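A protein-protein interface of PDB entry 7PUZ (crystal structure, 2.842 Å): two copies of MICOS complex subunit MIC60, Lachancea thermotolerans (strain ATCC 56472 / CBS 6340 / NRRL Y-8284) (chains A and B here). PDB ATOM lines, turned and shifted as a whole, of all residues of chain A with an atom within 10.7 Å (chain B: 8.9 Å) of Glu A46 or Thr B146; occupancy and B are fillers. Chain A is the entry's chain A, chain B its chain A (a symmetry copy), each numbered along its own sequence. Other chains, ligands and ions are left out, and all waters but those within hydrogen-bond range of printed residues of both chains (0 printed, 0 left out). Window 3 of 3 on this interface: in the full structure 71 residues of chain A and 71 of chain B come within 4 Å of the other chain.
Among the printed residues, merely in contact across the chains: Leu A39 with Leu B138 (3.5 Å), Leu A39 with Ser B139 (3.3 Å), Thr A40 with Leu B138 (3.8 Å), Phe A43 with Val B118 (3.7 Å), Phe A43 with Leu B141 (3.4 Å), Phe A43 with Ser B142 (3.8 Å), Phe A43 with Thr B145 (3.3 Å), Leu A44 with Val B118 (3.9 Å), Glu A46 with Thr B145 (3.2 Å), Phe A47 with Thr B145 (3.5 Å), Ala A49 with Lys B149 (3.6 Å), Phe A50 with Thr B145 (3.7 Å), Phe A50 with Lys B149 (3.7 Å), Phe A50 with Leu B169 (3.8 Å), Gln A53 with Leu B152 (3.7 Å) and Leu A54 with Leu B152 (3.5 Å).
No position is printed for both chains.
Of the 19 pairs that touch across the chains among the printed residues, none has its exchanged pair printed and touching as well.
Glu A38 touches none of the printed residues of chain B.
Of the printed residues of chain B, Leu A39 touches Leu B138 and Ser B139.
Glu A46 touches three residues of chain B.
Printed residues of chain B within 4 Å of Leu A54: Leu B152.
Of the printed residues of chain A, Leu B138 touches Leu A39 (3.5 Å) and Thr A40 (3.8 Å).
Of the printed residues of chain A, Leu B141 touches Phe A43.
Ser B142 touches just one residue of chain A: Phe A43 (3.8 Å).
Leu B144 touches none of the printed residues of chain A.
Thr B145 touches four residues of chain A.
Thr B146 touches just one residue of chain A: Glu A46.
No residue of chain A comes within 4 Å of Leu B147.
Of chain A, only Glu A46 (2.7 Å), Ala A49 (3.6 Å) and Phe A50 (3.7 Å) come within 4 Å of Lys B149.
Asn B150 touches none of the printed residues of chain A.
The nearest residue of chain B that does not touch Glu A46 is Ser B142 (4.6 Å).
The nearest residue of chain A that does not touch Thr B146 is Phe A50 (6.0 Å).
O of Leu A44 lies within hydrogen-bond range of ND2 of Asn A48 (2.9 Å).
The backbone carbonyl oxygen of Thr B146 lies close to the side-chain amide oxygen of Asn B150 (2.9 Å).
OG1 of Thr B146 is in hydrogen-bond range of O of Ser B142 (3.4 Å).
The side-chain hydroxyl of Thr B145 is in hydrogen-bond range of the backbone carbonyl oxygen of Leu B141 (3.0 Å).
The side-chain amide nitrogen (NE2) of Gln A53 is in hydrogen-bond range of a ring nitrogen (NE2) of His B153, 3.1 Å away.
The side-chain hydroxyl (OG1) of Thr B146 lies close to the side-chain carboxylate (OE1) of Glu A46, at 2.3 Å.
The side-chain carboxylate of Glu A46 lies within salt-bridge range of the side-chain amino group of Lys B149, at 2.7 Å.
Hydrophobic or aromatic side chains of chain B that line the printed part of chain A: Val B118, Leu B138, Leu B141, Leu B152, His B153 and Leu B169.
Hydrophobic or aromatic side chains of chain A that line the printed part of chain B: Leu A39, Phe A43, Leu A44, Ala A49, Phe A50 and Leu A54.
Among the printed residues, 19 pairs touch across the chains.
Among the printed residues, Asp or Glu carboxylates within 4 Å of a Lys or Arg side-chain nitrogen of the other chain: Glu A46 with Lys B149 (2.7 Å).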
ATOM      1  N   GLU A  38       3.204 -29.112   0.250  1.00  0.00           N
ATOM      2  CA  GLU A  38       4.641 -29.159  -0.011  1.00  0.00           C
ATOM      3  C   GLU A  38       5.381 -28.112   0.817  1.00  0.00           C
ATOM      4  O   GLU A  38       6.405 -28.407   1.452  1.00  0.00           O
ATOM      5  CB  GLU A  38       4.904 -28.963  -1.506  1.00  0.00           C
ATOM      6  CG  GLU A  38       6.296 -29.378  -1.955  1.00  0.00           C
ATOM      7  CD  GLU A  38       6.527 -29.156  -3.443  1.00  0.00           C
ATOM      8  OE1 GLU A  38       5.591 -28.686  -4.131  1.00  0.00           O
ATOM      9  OE2 GLU A  38       7.648 -29.450  -3.923  1.00  0.00           O
ATOM     10  N   LEU A  39       4.859 -26.883   0.844  1.00  0.00           N
ATOM     11  CA  LEU A  39       5.514 -25.815   1.593  1.00  0.00           C
ATOM     12  C   LEU A  39       5.449 -26.061   3.099  1.00  0.00           C
ATOM     13  O   LEU A  39       6.406 -25.760   3.822  1.00  0.00           O
ATOM     14  CB  LEU A  39       4.887 -24.468   1.241  1.00  0.00           C
ATOM     15  CG  LEU A  39       5.141 -23.867  -0.138  1.00  0.00           C
ATOM     16  CD1 LEU A  39       4.833 -22.383  -0.117  1.00  0.00           C
ATOM     17  CD2 LEU A  39       6.571 -24.119  -0.586  1.00  0.00           C
ATOM     18  N   THR A  40       4.327 -26.591   3.595  1.00  0.00           N
ATOM     19  CA  THR A  40       4.228 -26.924   5.012  1.00  0.00           C
ATOM     20  C   THR A  40       5.254 -27.982   5.389  1.00  0.00           C
ATOM     21  O   THR A  40       5.874 -27.908   6.456  1.00  0.00           O
ATOM     22  CB  THR A  40       2.813 -27.406   5.341  1.00  0.00           C
ATOM     23  OG1 THR A  40       1.875 -26.371   5.040  1.00  0.00           O
ATOM     24  CG2 THR A  40       2.684 -27.768   6.811  1.00  0.00           C
ATOM     25  N   GLN A  41       5.454 -28.965   4.514  1.00  0.00           N
ATOM     26  CA  GLN A  41       6.456 -29.992   4.762  1.00  0.00           C
ATOM     27  C   GLN A  41       7.855 -29.387   4.821  1.00  0.00           C
ATOM     28  O   GLN A  41       8.646 -29.688   5.731  1.00  0.00           O
ATOM     29  CB  GLN A  41       6.359 -31.049   3.666  1.00  0.00           C
ATOM     30  CG  GLN A  41       6.643 -32.451   4.114  1.00  0.00           C
ATOM     31  CD  GLN A  41       6.370 -33.465   3.030  1.00  0.00           C
ATOM     32  OE1 GLN A  41       6.019 -33.110   1.906  1.00  0.00           O
ATOM     33  NE2 GLN A  41       6.527 -34.740   3.359  1.00  0.00           N
ATOM     34  N   GLN A  42       8.178 -28.531   3.846  1.00  0.00           N
ATOM     35  CA  GLN A  42       9.485 -27.880   3.843  1.00  0.00           C
ATOM     36  C   GLN A  42       9.691 -27.056   5.107  1.00  0.00           C
ATOM     37  O   GLN A  42      10.770 -27.093   5.710  1.00  0.00           O
ATOM     38  CB  GLN A  42       9.646 -27.003   2.604  1.00  0.00           C
ATOM     39  CG  GLN A  42       9.870 -27.772   1.318  1.00  0.00           C
ATOM     40  CD  GLN A  42       9.841 -26.872   0.094  1.00  0.00           C
ATOM     41  OE1 GLN A  42       9.842 -25.645   0.213  1.00  0.00           O
ATOM     42  NE2 GLN A  42       9.804 -27.479  -1.092  1.00  0.00           N
ATOM     43  N   PHE A  43       8.667 -26.310   5.526  1.00  0.00           N
ATOM     44  CA  PHE A  43       8.803 -25.502   6.731  1.00  0.00           C
ATOM     45  C   PHE A  43       8.942 -26.374   7.970  1.00  0.00           C
ATOM     46  O   PHE A  43       9.692 -26.030   8.886  1.00  0.00           O
ATOM     47  CB  PHE A  43       7.622 -24.549   6.887  1.00  0.00           C
ATOM     48  CG  PHE A  43       7.603 -23.836   8.207  1.00  0.00           C
ATOM     49  CD1 PHE A  43       8.704 -23.103   8.627  1.00  0.00           C
ATOM     50  CD2 PHE A  43       6.496 -23.908   9.035  1.00  0.00           C
ATOM     51  CE1 PHE A  43       8.698 -22.451   9.847  1.00  0.00           C
ATOM     52  CE2 PHE A  43       6.481 -23.255  10.254  1.00  0.00           C
ATOM     53  CZ  PHE A  43       7.586 -22.528  10.661  1.00  0.00           C
ATOM     54  N   LEU A  44       8.229 -27.500   8.024  1.00  0.00           N
ATOM     55  CA  LEU A  44       8.377 -28.413   9.152  1.00  0.00           C
ATOM     56  C   LEU A  44       9.816 -28.886   9.277  1.00  0.00           C
ATOM     57  O   LEU A  44      10.417 -28.822  10.361  1.00  0.00           O
ATOM     58  CB  LEU A  44       7.437 -29.606   8.990  1.00  0.00           C
ATOM     59  CG  LEU A  44       6.191 -29.633   9.874  1.00  0.00           C
ATOM     60  CD1 LEU A  44       5.423 -30.935   9.671  1.00  0.00           C
ATOM     61  CD2 LEU A  44       6.567 -29.458  11.339  1.00  0.00           C
ATOM     62  N   ASN A  45      10.387 -29.360   8.168  1.00  0.00           N
ATOM     63  CA  ASN A  45      11.754 -29.869   8.214  1.00  0.00           C
ATOM     64  C   ASN A  45      12.749 -28.766   8.556  1.00  0.00           C
ATOM     65  O   ASN A  45      13.628 -28.963   9.405  1.00  0.00           O
ATOM     66  CB  ASN A  45      12.116 -30.536   6.888  1.00  0.00           C
ATOM     67  CG  ASN A  45      11.414 -31.871   6.696  1.00  0.00           C
ATOM     68  OD1 ASN A  45      11.173 -32.604   7.656  1.00  0.00           O
ATOM     69  ND2 ASN A  45      11.081 -32.190   5.450  1.00  0.00           N
ATOM     70  N   GLU A  46      12.627 -27.597   7.917  1.00  0.00           N
ATOM     71  CA  GLU A  46      13.546 -26.505   8.224  1.00  0.00           C
ATOM     72  C   GLU A  46      13.408 -26.047   9.669  1.00  0.00           C
ATOM     73  O   GLU A  46      14.414 -25.714  10.307  1.00  0.00           O
ATOM     74  CB  GLU A  46      13.319 -25.333   7.268  1.00  0.00           C
ATOM     75  CG  GLU A  46      13.795 -25.592   5.848  1.00  0.00           C
ATOM     76  CD  GLU A  46      15.300 -25.758   5.760  1.00  0.00           C
ATOM     77  OE1 GLU A  46      15.998 -24.753   5.500  1.00  0.00           O
ATOM     78  OE2 GLU A  46      15.791 -26.891   5.959  1.00  0.00           O
ATOM     79  N   PHE A  47      12.190 -26.043  10.216  1.00  0.00           N
ATOM     80  CA  PHE A  47      12.014 -25.593  11.590  1.00  0.00           C
ATOM     81  C   PHE A  47      12.612 -26.581  12.571  1.00  0.00           C
ATOM     82  O   PHE A  47      13.231 -26.177  13.555  1.00  0.00           O
ATOM     83  CB  PHE A  47      10.537 -25.375  11.913  1.00  0.00           C
ATOM     84  CG  PHE A  47      10.298 -24.968  13.340  1.00  0.00           C
ATOM     85  CD1 PHE A  47      10.570 -23.675  13.756  1.00  0.00           C
ATOM     86  CD2 PHE A  47       9.831 -25.882  14.270  1.00  0.00           C
ATOM     87  CE1 PHE A  47      10.365 -23.296  15.071  1.00  0.00           C
ATOM     88  CE2 PHE A  47       9.624 -25.508  15.585  1.00  0.00           C
ATOM     89  CZ  PHE A  47       9.892 -24.214  15.985  1.00  0.00           C
ATOM     90  N   ASN A  48      12.433 -27.881  12.332  1.00  0.00           N
ATOM     91  CA  ASN A  48      13.032 -28.846  13.245  1.00  0.00           C
ATOM     92  C   ASN A  48      14.551 -28.846  13.132  1.00  0.00           C
ATOM     93  O   ASN A  48      15.244 -29.058  14.137  1.00  0.00           O
ATOM     94  CB  ASN A  48      12.459 -30.240  12.997  1.00  0.00           C
ATOM     95  CG  ASN A  48      11.094 -30.427  13.640  1.00  0.00           C
ATOM     96  OD1 ASN A  48      10.989 -30.915  14.769  1.00  0.00           O
ATOM     97  ND2 ASN A  48      10.042 -30.021  12.929  1.00  0.00           N
ATOM     98  N   ALA A  49      15.088 -28.587  11.936  1.00  0.00           N
ATOM     99  CA  ALA A  49      16.533 -28.440  11.803  1.00  0.00           C
ATOM    100  C   ALA A  49      17.037 -27.244  12.605  1.00  0.00           C
ATOM    101  O   ALA A  49      17.997 -27.362  13.380  1.00  0.00           O
ATOM    102  CB  ALA A  49      16.911 -28.311  10.328  1.00  0.00           C
ATOM    103  N   PHE A  50      16.400 -26.081  12.429  1.00  0.00           N
ATOM    104  CA  PHE A  50      16.775 -24.896  13.197  1.00  0.00           C
ATOM    105  C   PHE A  50      16.640 -25.142  14.694  1.00  0.00           C
ATOM    106  O   PHE A  50      17.468 -24.679  15.490  1.00  0.00           O
ATOM    107  CB  PHE A  50      15.913 -23.709  12.765  1.00  0.00           C
ATOM    108  CG  PHE A  50      15.772 -22.644  13.814  1.00  0.00           C
ATOM    109  CD1 PHE A  50      16.853 -21.854  14.173  1.00  0.00           C
ATOM    110  CD2 PHE A  50      14.550 -22.416  14.426  1.00  0.00           C
ATOM    111  CE1 PHE A  50      16.719 -20.867  15.133  1.00  0.00           C
ATOM    112  CE2 PHE A  50      14.411 -21.434  15.384  1.00  0.00           C
ATOM    113  CZ  PHE A  50      15.497 -20.658  15.741  1.00  0.00           C
ATOM    114  N   LYS A  51      15.605 -25.885  15.091  1.00  0.00           N
ATOM    115  CA  LYS A  51      15.349 -26.147  16.501  1.00  0.00           C
ATOM    116  C   LYS A  51      16.454 -26.999  17.104  1.00  0.00           C
ATOM    117  O   LYS A  51      17.012 -26.662  18.157  1.00  0.00           O
ATOM    118  CB  LYS A  51      13.990 -26.831  16.645  1.00  0.00           C
ATOM    119  CG  LYS A  51      13.504 -27.020  18.060  1.00  0.00           C
ATOM    120  CD  LYS A  51      12.069 -27.531  18.052  1.00  0.00           C
ATOM    121  CE  LYS A  51      11.564 -27.766  19.466  1.00  0.00           C
ATOM    122  NZ  LYS A  51      12.413 -28.759  20.188  1.00  0.00           N
ATOM    123  N   ALA A  52      16.777 -28.117  16.449  1.00  0.00           N
ATOM    124  CA  ALA A  52      17.864 -28.961  16.929  1.00  0.00           C
ATOM    125  C   ALA A  52      19.182 -28.205  16.948  1.00  0.00           C
ATOM    126  O   ALA A  52      19.974 -28.368  17.881  1.00  0.00           O
ATOM    127  CB  ALA A  52      17.981 -30.213  16.063  1.00  0.00           C
ATOM    128  N   GLN A  53      19.424 -27.358  15.947  1.00  0.00           N
ATOM    129  CA  GLN A  53      20.670 -26.603  15.902  1.00  0.00           C
ATOM    130  C   GLN A  53      20.779 -25.656  17.092  1.00  0.00           C
ATOM    131  O   GLN A  53      21.803 -25.623  17.790  1.00  0.00           O
ATOM    132  CB  GLN A  53      20.754 -25.837  14.581  1.00  0.00           C
ATOM    133  CG  GLN A  53      22.147 -25.385  14.219  1.00  0.00           C
ATOM    134  CD  GLN A  53      23.072 -26.547  13.950  1.00  0.00           C
ATOM    135  OE1 GLN A  53      23.903 -26.900  14.787  1.00  0.00           O
ATOM    136  NE2 GLN A  53      22.933 -27.155  12.778  1.00  0.00           N
ATOM    137  N   LEU A  54      19.723 -24.873  17.337  1.00  0.00           N
ATOM    138  CA  LEU A  54      19.738 -23.921  18.443  1.00  0.00           C
ATOM    139  C   LEU A  54      19.883 -24.637  19.780  1.00  0.00           C
ATOM    140  O   LEU A  54      20.666 -24.216  20.644  1.00  0.00           O
ATOM    141  CB  LEU A  54      18.465 -23.072  18.408  1.00  0.00           C
ATOM    142  CG  LEU A  54      18.289 -21.944  19.422  1.00  0.00           C
ATOM    143  CD1 LEU A  54      19.522 -21.062  19.470  1.00  0.00           C
ATOM    144  CD2 LEU A  54      17.064 -21.120  19.062  1.00  0.00           C
ATOM    145  N   VAL B 118       3.625 -24.576  15.515  1.00  0.00           N
ATOM    146  CA  VAL B 118       3.994 -25.063  14.187  1.00  0.00           C
ATOM    147  C   VAL B 118       3.391 -26.440  13.940  1.00  0.00           C
ATOM    148  O   VAL B 118       2.833 -26.710  12.868  1.00  0.00           O
ATOM    149  CB  VAL B 118       5.524 -25.077  14.027  1.00  0.00           C
ATOM    150  CG1 VAL B 118       5.925 -25.877  12.798  1.00  0.00           C
ATOM    151  CG2 VAL B 118       6.053 -23.660  13.924  1.00  0.00           C
ATOM    152  N   LEU B 138       3.745 -18.144   4.687  1.00  0.00           N
ATOM    153  CA  LEU B 138       4.390 -19.442   4.879  1.00  0.00           C
ATOM    154  C   LEU B 138       5.773 -19.471   4.242  1.00  0.00           C
ATOM    155  O   LEU B 138       6.741 -19.938   4.854  1.00  0.00           O
ATOM    156  CB  LEU B 138       3.514 -20.555   4.309  1.00  0.00           C
ATOM    157  CG  LEU B 138       4.099 -21.953   4.461  1.00  0.00           C
ATOM    158  CD1 LEU B 138       4.341 -22.288   5.924  1.00  0.00           C
ATOM    159  CD2 LEU B 138       3.165 -22.964   3.828  1.00  0.00           C
ATOM    160  N   SER B 139       5.882 -18.978   3.005  1.00  0.00           N
ATOM    161  CA  SER B 139       7.173 -18.931   2.329  1.00  0.00           C
ATOM    162  C   SER B 139       8.143 -18.004   3.053  1.00  0.00           C
ATOM    163  O   SER B 139       9.331 -18.318   3.191  1.00  0.00           O
ATOM    164  CB  SER B 139       6.989 -18.493   0.873  1.00  0.00           C
ATOM    165  OG  SER B 139       6.690 -19.599   0.035  1.00  0.00           O
ATOM    166  N   GLN B 140       7.649 -16.855   3.525  1.00  0.00           N
ATOM    167  CA  GLN B 140       8.515 -15.933   4.255  1.00  0.00           C
ATOM    168  C   GLN B 140       9.036 -16.565   5.542  1.00  0.00           C
ATOM    169  O   GLN B 140      10.235 -16.492   5.840  1.00  0.00           O
ATOM    170  CB  GLN B 140       7.758 -14.639   4.554  1.00  0.00           C
ATOM    171  CG  GLN B 140       8.638 -13.516   5.074  1.00  0.00           C
ATOM    172  CD  GLN B 140       7.937 -12.175   5.055  1.00  0.00           C
ATOM    173  OE1 GLN B 140       6.849 -12.040   4.495  1.00  0.00           O
ATOM    174  NE2 GLN B 140       8.558 -11.172   5.662  1.00  0.00           N
ATOM    175  N   LEU B 141       8.147 -17.201   6.311  1.00  0.00           N
ATOM    176  CA  LEU B 141       8.547 -17.874   7.543  1.00  0.00           C
ATOM    177  C   LEU B 141       9.518 -19.019   7.272  1.00  0.00           C
ATOM    178  O   LEU B 141      10.480 -19.207   8.026  1.00  0.00           O
ATOM    179  CB  LEU B 141       7.298 -18.375   8.270  1.00  0.00           C
ATOM    180  CG  LEU B 141       7.391 -19.139   9.589  1.00  0.00           C
ATOM    181  CD1 LEU B 141       8.051 -18.306  10.672  1.00  0.00           C
ATOM    182  CD2 LEU B 141       5.995 -19.565  10.023  1.00  0.00           C
ATOM    183  N   SER B 142       9.294 -19.780   6.197  1.00  0.00           N
ATOM    184  CA  SER B 142      10.194 -20.876   5.848  1.00  0.00           C
ATOM    185  C   SER B 142      11.592 -20.354   5.528  1.00  0.00           C
ATOM    186  O   SER B 142      12.598 -20.857   6.053  1.00  0.00           O
ATOM    187  CB  SER B 142       9.613 -21.657   4.665  1.00  0.00           C
ATOM    188  OG  SER B 142      10.300 -22.870   4.444  1.00  0.00           O
ATOM    189  N   LEU B 143      11.676 -19.337   4.665  1.00  0.00           N
ATOM    190  CA  LEU B 143      12.981 -18.779   4.318  1.00  0.00           C
ATOM    191  C   LEU B 143      13.660 -18.157   5.533  1.00  0.00           C
ATOM    192  O   LEU B 143      14.890 -18.211   5.662  1.00  0.00           O
ATOM    193  CB  LEU B 143      12.842 -17.752   3.195  1.00  0.00           C
ATOM    194  CG  LEU B 143      14.140 -17.049   2.790  1.00  0.00           C
ATOM    195  CD1 LEU B 143      15.205 -18.062   2.386  1.00  0.00           C
ATOM    196  CD2 LEU B 143      13.887 -16.049   1.670  1.00  0.00           C
ATOM    197  N   LEU B 144      12.880 -17.558   6.436  1.00  0.00           N
ATOM    198  CA  LEU B 144      13.467 -17.004   7.651  1.00  0.00           C
ATOM    199  C   LEU B 144      14.041 -18.105   8.529  1.00  0.00           C
ATOM    200  O   LEU B 144      15.138 -17.961   9.082  1.00  0.00           O
ATOM    201  CB  LEU B 144      12.423 -16.196   8.418  1.00  0.00           C
ATOM    202  CG  LEU B 144      12.919 -15.513   9.694  1.00  0.00           C
ATOM    203  CD1 LEU B 144      14.231 -14.788   9.436  1.00  0.00           C
ATOM    204  CD2 LEU B 144      11.868 -14.547  10.231  1.00  0.00           C
ATOM    205  N   THR B 145      13.314 -19.215   8.668  1.00  0.00           N
ATOM    206  CA  THR B 145      13.846 -20.346   9.418  1.00  0.00           C
ATOM    207  C   THR B 145      15.145 -20.842   8.803  1.00  0.00           C
ATOM    208  O   THR B 145      16.092 -21.183   9.520  1.00  0.00           O
ATOM    209  CB  THR B 145      12.819 -21.474   9.468  1.00  0.00           C
ATOM    210  OG1 THR B 145      11.633 -21.004  10.116  1.00  0.00           O
ATOM    211  CG2 THR B 145      13.374 -22.657  10.234  1.00  0.00           C
ATOM    212  N   THR B 146      15.209 -20.883   7.474  1.00  0.00           N
ATOM    213  CA  THR B 146      16.431 -21.337   6.814  1.00  0.00           C
ATOM    214  C   THR B 146      17.594 -20.390   7.095  1.00  0.00           C
ATOM    215  O   THR B 146      18.691 -20.827   7.472  1.00  0.00           O
ATOM    216  CB  THR B 146      16.189 -21.472   5.315  1.00  0.00           C
ATOM    217  OG1 THR B 146      15.346 -22.607   5.084  1.00  0.00           O
ATOM    218  CG2 THR B 146      17.502 -21.657   4.574  1.00  0.00           C
ATOM    219  N   LEU B 147      17.369 -19.087   6.903  1.00  0.00           N
ATOM    220  CA  LEU B 147      18.376 -18.081   7.230  1.00  0.00           C
ATOM    221  C   LEU B 147      18.881 -18.247   8.658  1.00  0.00           C
ATOM    222  O   LEU B 147      20.092 -18.222   8.912  1.00  0.00           O
ATOM    223  CB  LEU B 147      17.793 -16.677   7.039  1.00  0.00           C
ATOM    224  CG  LEU B 147      17.961 -15.926   5.716  1.00  0.00           C
ATOM    225  CD1 LEU B 147      17.064 -14.705   5.716  1.00  0.00           C
ATOM    226  CD2 LEU B 147      19.412 -15.520   5.512  1.00  0.00           C
ATOM    227  N   LEU B 148      17.955 -18.432   9.603  1.00  0.00           N
ATOM    228  CA  LEU B 148      18.332 -18.537  11.010  1.00  0.00           C
ATOM    229  C   LEU B 148      19.146 -19.799  11.273  1.00  0.00           C
ATOM    230  O   LEU B 148      20.181 -19.750  11.946  1.00  0.00           O
ATOM    231  CB  LEU B 148      17.082 -18.506  11.886  1.00  0.00           C
ATOM    232  CG  LEU B 148      16.823 -17.194  12.611  1.00  0.00           C
ATOM    233  CD1 LEU B 148      16.918 -16.014  11.660  1.00  0.00           C
ATOM    234  CD2 LEU B 148      15.465 -17.232  13.295  1.00  0.00           C
ATOM    235  N   LYS B 149      18.694 -20.939  10.752  1.00  0.00           N
ATOM    236  CA  LYS B 149      19.431 -22.183  10.944  1.00  0.00           C
ATOM    237  C   LYS B 149      20.826 -22.108  10.341  1.00  0.00           C
ATOM    238  O   LYS B 149      21.769 -22.696  10.884  1.00  0.00           O
ATOM    239  CB  LYS B 149      18.647 -23.350  10.343  1.00  0.00           C
ATOM    240  CG  LYS B 149      19.506 -24.431   9.708  1.00  0.00           C
ATOM    241  CD  LYS B 149      18.643 -25.458   9.010  1.00  0.00           C
ATOM    242  CE  LYS B 149      19.206 -25.809   7.642  1.00  0.00           C
ATOM    243  NZ  LYS B 149      18.311 -26.746   6.896  1.00  0.00           N
ATOM    244  N   ASN B 150      20.985 -21.383   9.233  1.00  0.00           N
ATOM    245  CA  ASN B 150      22.291 -21.301   8.591  1.00  0.00           C
ATOM    246  C   ASN B 150      23.186 -20.218   9.180  1.00  0.00           C
ATOM    247  O   ASN B 150      24.398 -20.238   8.939  1.00  0.00           O
ATOM    248  CB  ASN B 150      22.130 -21.076   7.085  1.00  0.00           C
ATOM    249  CG  ASN B 150      21.546 -22.285   6.378  1.00  0.00           C
ATOM    250  OD1 ASN B 150      20.527 -22.186   5.696  1.00  0.00           O
ATOM    251  ND2 ASN B 150      22.187 -23.435   6.545  1.00  0.00           N
ATOM    252  N   LYS B 151      22.629 -19.273   9.937  1.00  0.00           N
ATOM    253  CA  LYS B 151      23.479 -18.383  10.721  1.00  0.00           C
ATOM    254  C   LYS B 151      24.040 -19.075  11.955  1.00  0.00           C
ATOM    255  O   LYS B 151      25.023 -18.592  12.530  1.00  0.00           O
ATOM    256  CB  LYS B 151      22.711 -17.132  11.147  1.00  0.00           C
ATOM    257  CG  LYS B 151      22.329 -16.205  10.012  1.00  0.00           C
ATOM    258  CD  LYS B 151      21.746 -14.905  10.562  1.00  0.00           C
ATOM    259  CE  LYS B 151      21.097 -14.056   9.473  1.00  0.00           C
ATOM    260  NZ  LYS B 151      20.518 -12.790  10.015  1.00  0.00           N
ATOM    261  N   LEU B 152      23.441 -20.192  12.368  1.00  0.00           N
ATOM    262  CA  LEU B 152      23.831 -20.906  13.577  1.00  0.00           C
ATOM    263  C   LEU B 152      24.989 -21.860  13.361  1.00  0.00           C
ATOM    264  O   LEU B 152      25.242 -22.702  14.228  1.00  0.00           O
ATOM    265  CB  LEU B 152      22.644 -21.683  14.142  1.00  0.00           C
ATOM    266  CG  LEU B 152      21.746 -20.928  15.114  1.00  0.00           C
ATOM    267  CD1 LEU B 152      20.764 -21.885  15.759  1.00  0.00           C
ATOM    268  CD2 LEU B 152      22.584 -20.218  16.160  1.00  0.00           C
ATOM    269  N   HIS B 153      25.677 -21.773  12.233  1.00  0.00           N
ATOM    270  CA  HIS B 153      26.864 -22.578  11.979  1.00  0.00           C
ATOM    271  C   HIS B 153      28.081 -21.704  12.254  1.00  0.00           C
ATOM    272  O   HIS B 153      28.469 -20.887  11.413  1.00  0.00           O
ATOM    273  CB  HIS B 153      26.857 -23.112  10.549  1.00  0.00           C
ATOM    274  CG  HIS B 153      25.753 -24.079  10.285  1.00  0.00           C
ATOM    275  ND1 HIS B 153      25.379 -24.462   9.007  1.00  0.00           N
ATOM    276  CD2 HIS B 153      24.931 -24.752  11.123  1.00  0.00           C
ATOM    277  CE1 HIS B 153      24.384 -25.318   9.080  1.00  0.00           C
ATOM    278  NE2 HIS B 153      24.088 -25.515  10.358  1.00  0.00           N
ATOM    279  N   LEU B 169       9.634 -14.942  14.164  1.00  0.00           N
ATOM    280  CA  LEU B 169       9.045 -16.266  13.971  1.00  0.00           C
ATOM    281  C   LEU B 169       7.685 -16.367  14.647  1.00  0.00           C
ATOM    282  O   LEU B 169       6.673 -16.649  13.994  1.00  0.00           O
ATOM    283  CB  LEU B 169       9.986 -17.344  14.514  1.00  0.00           C
ATOM    284  CG  LEU B 169      11.299 -17.629  13.782  1.00  0.00           C
ATOM    285  CD1 LEU B 169      11.761 -19.041  14.086  1.00  0.00           C
ATOM    286  CD2 LEU B 169      11.138 -17.442  12.297  1.00  0.00           C
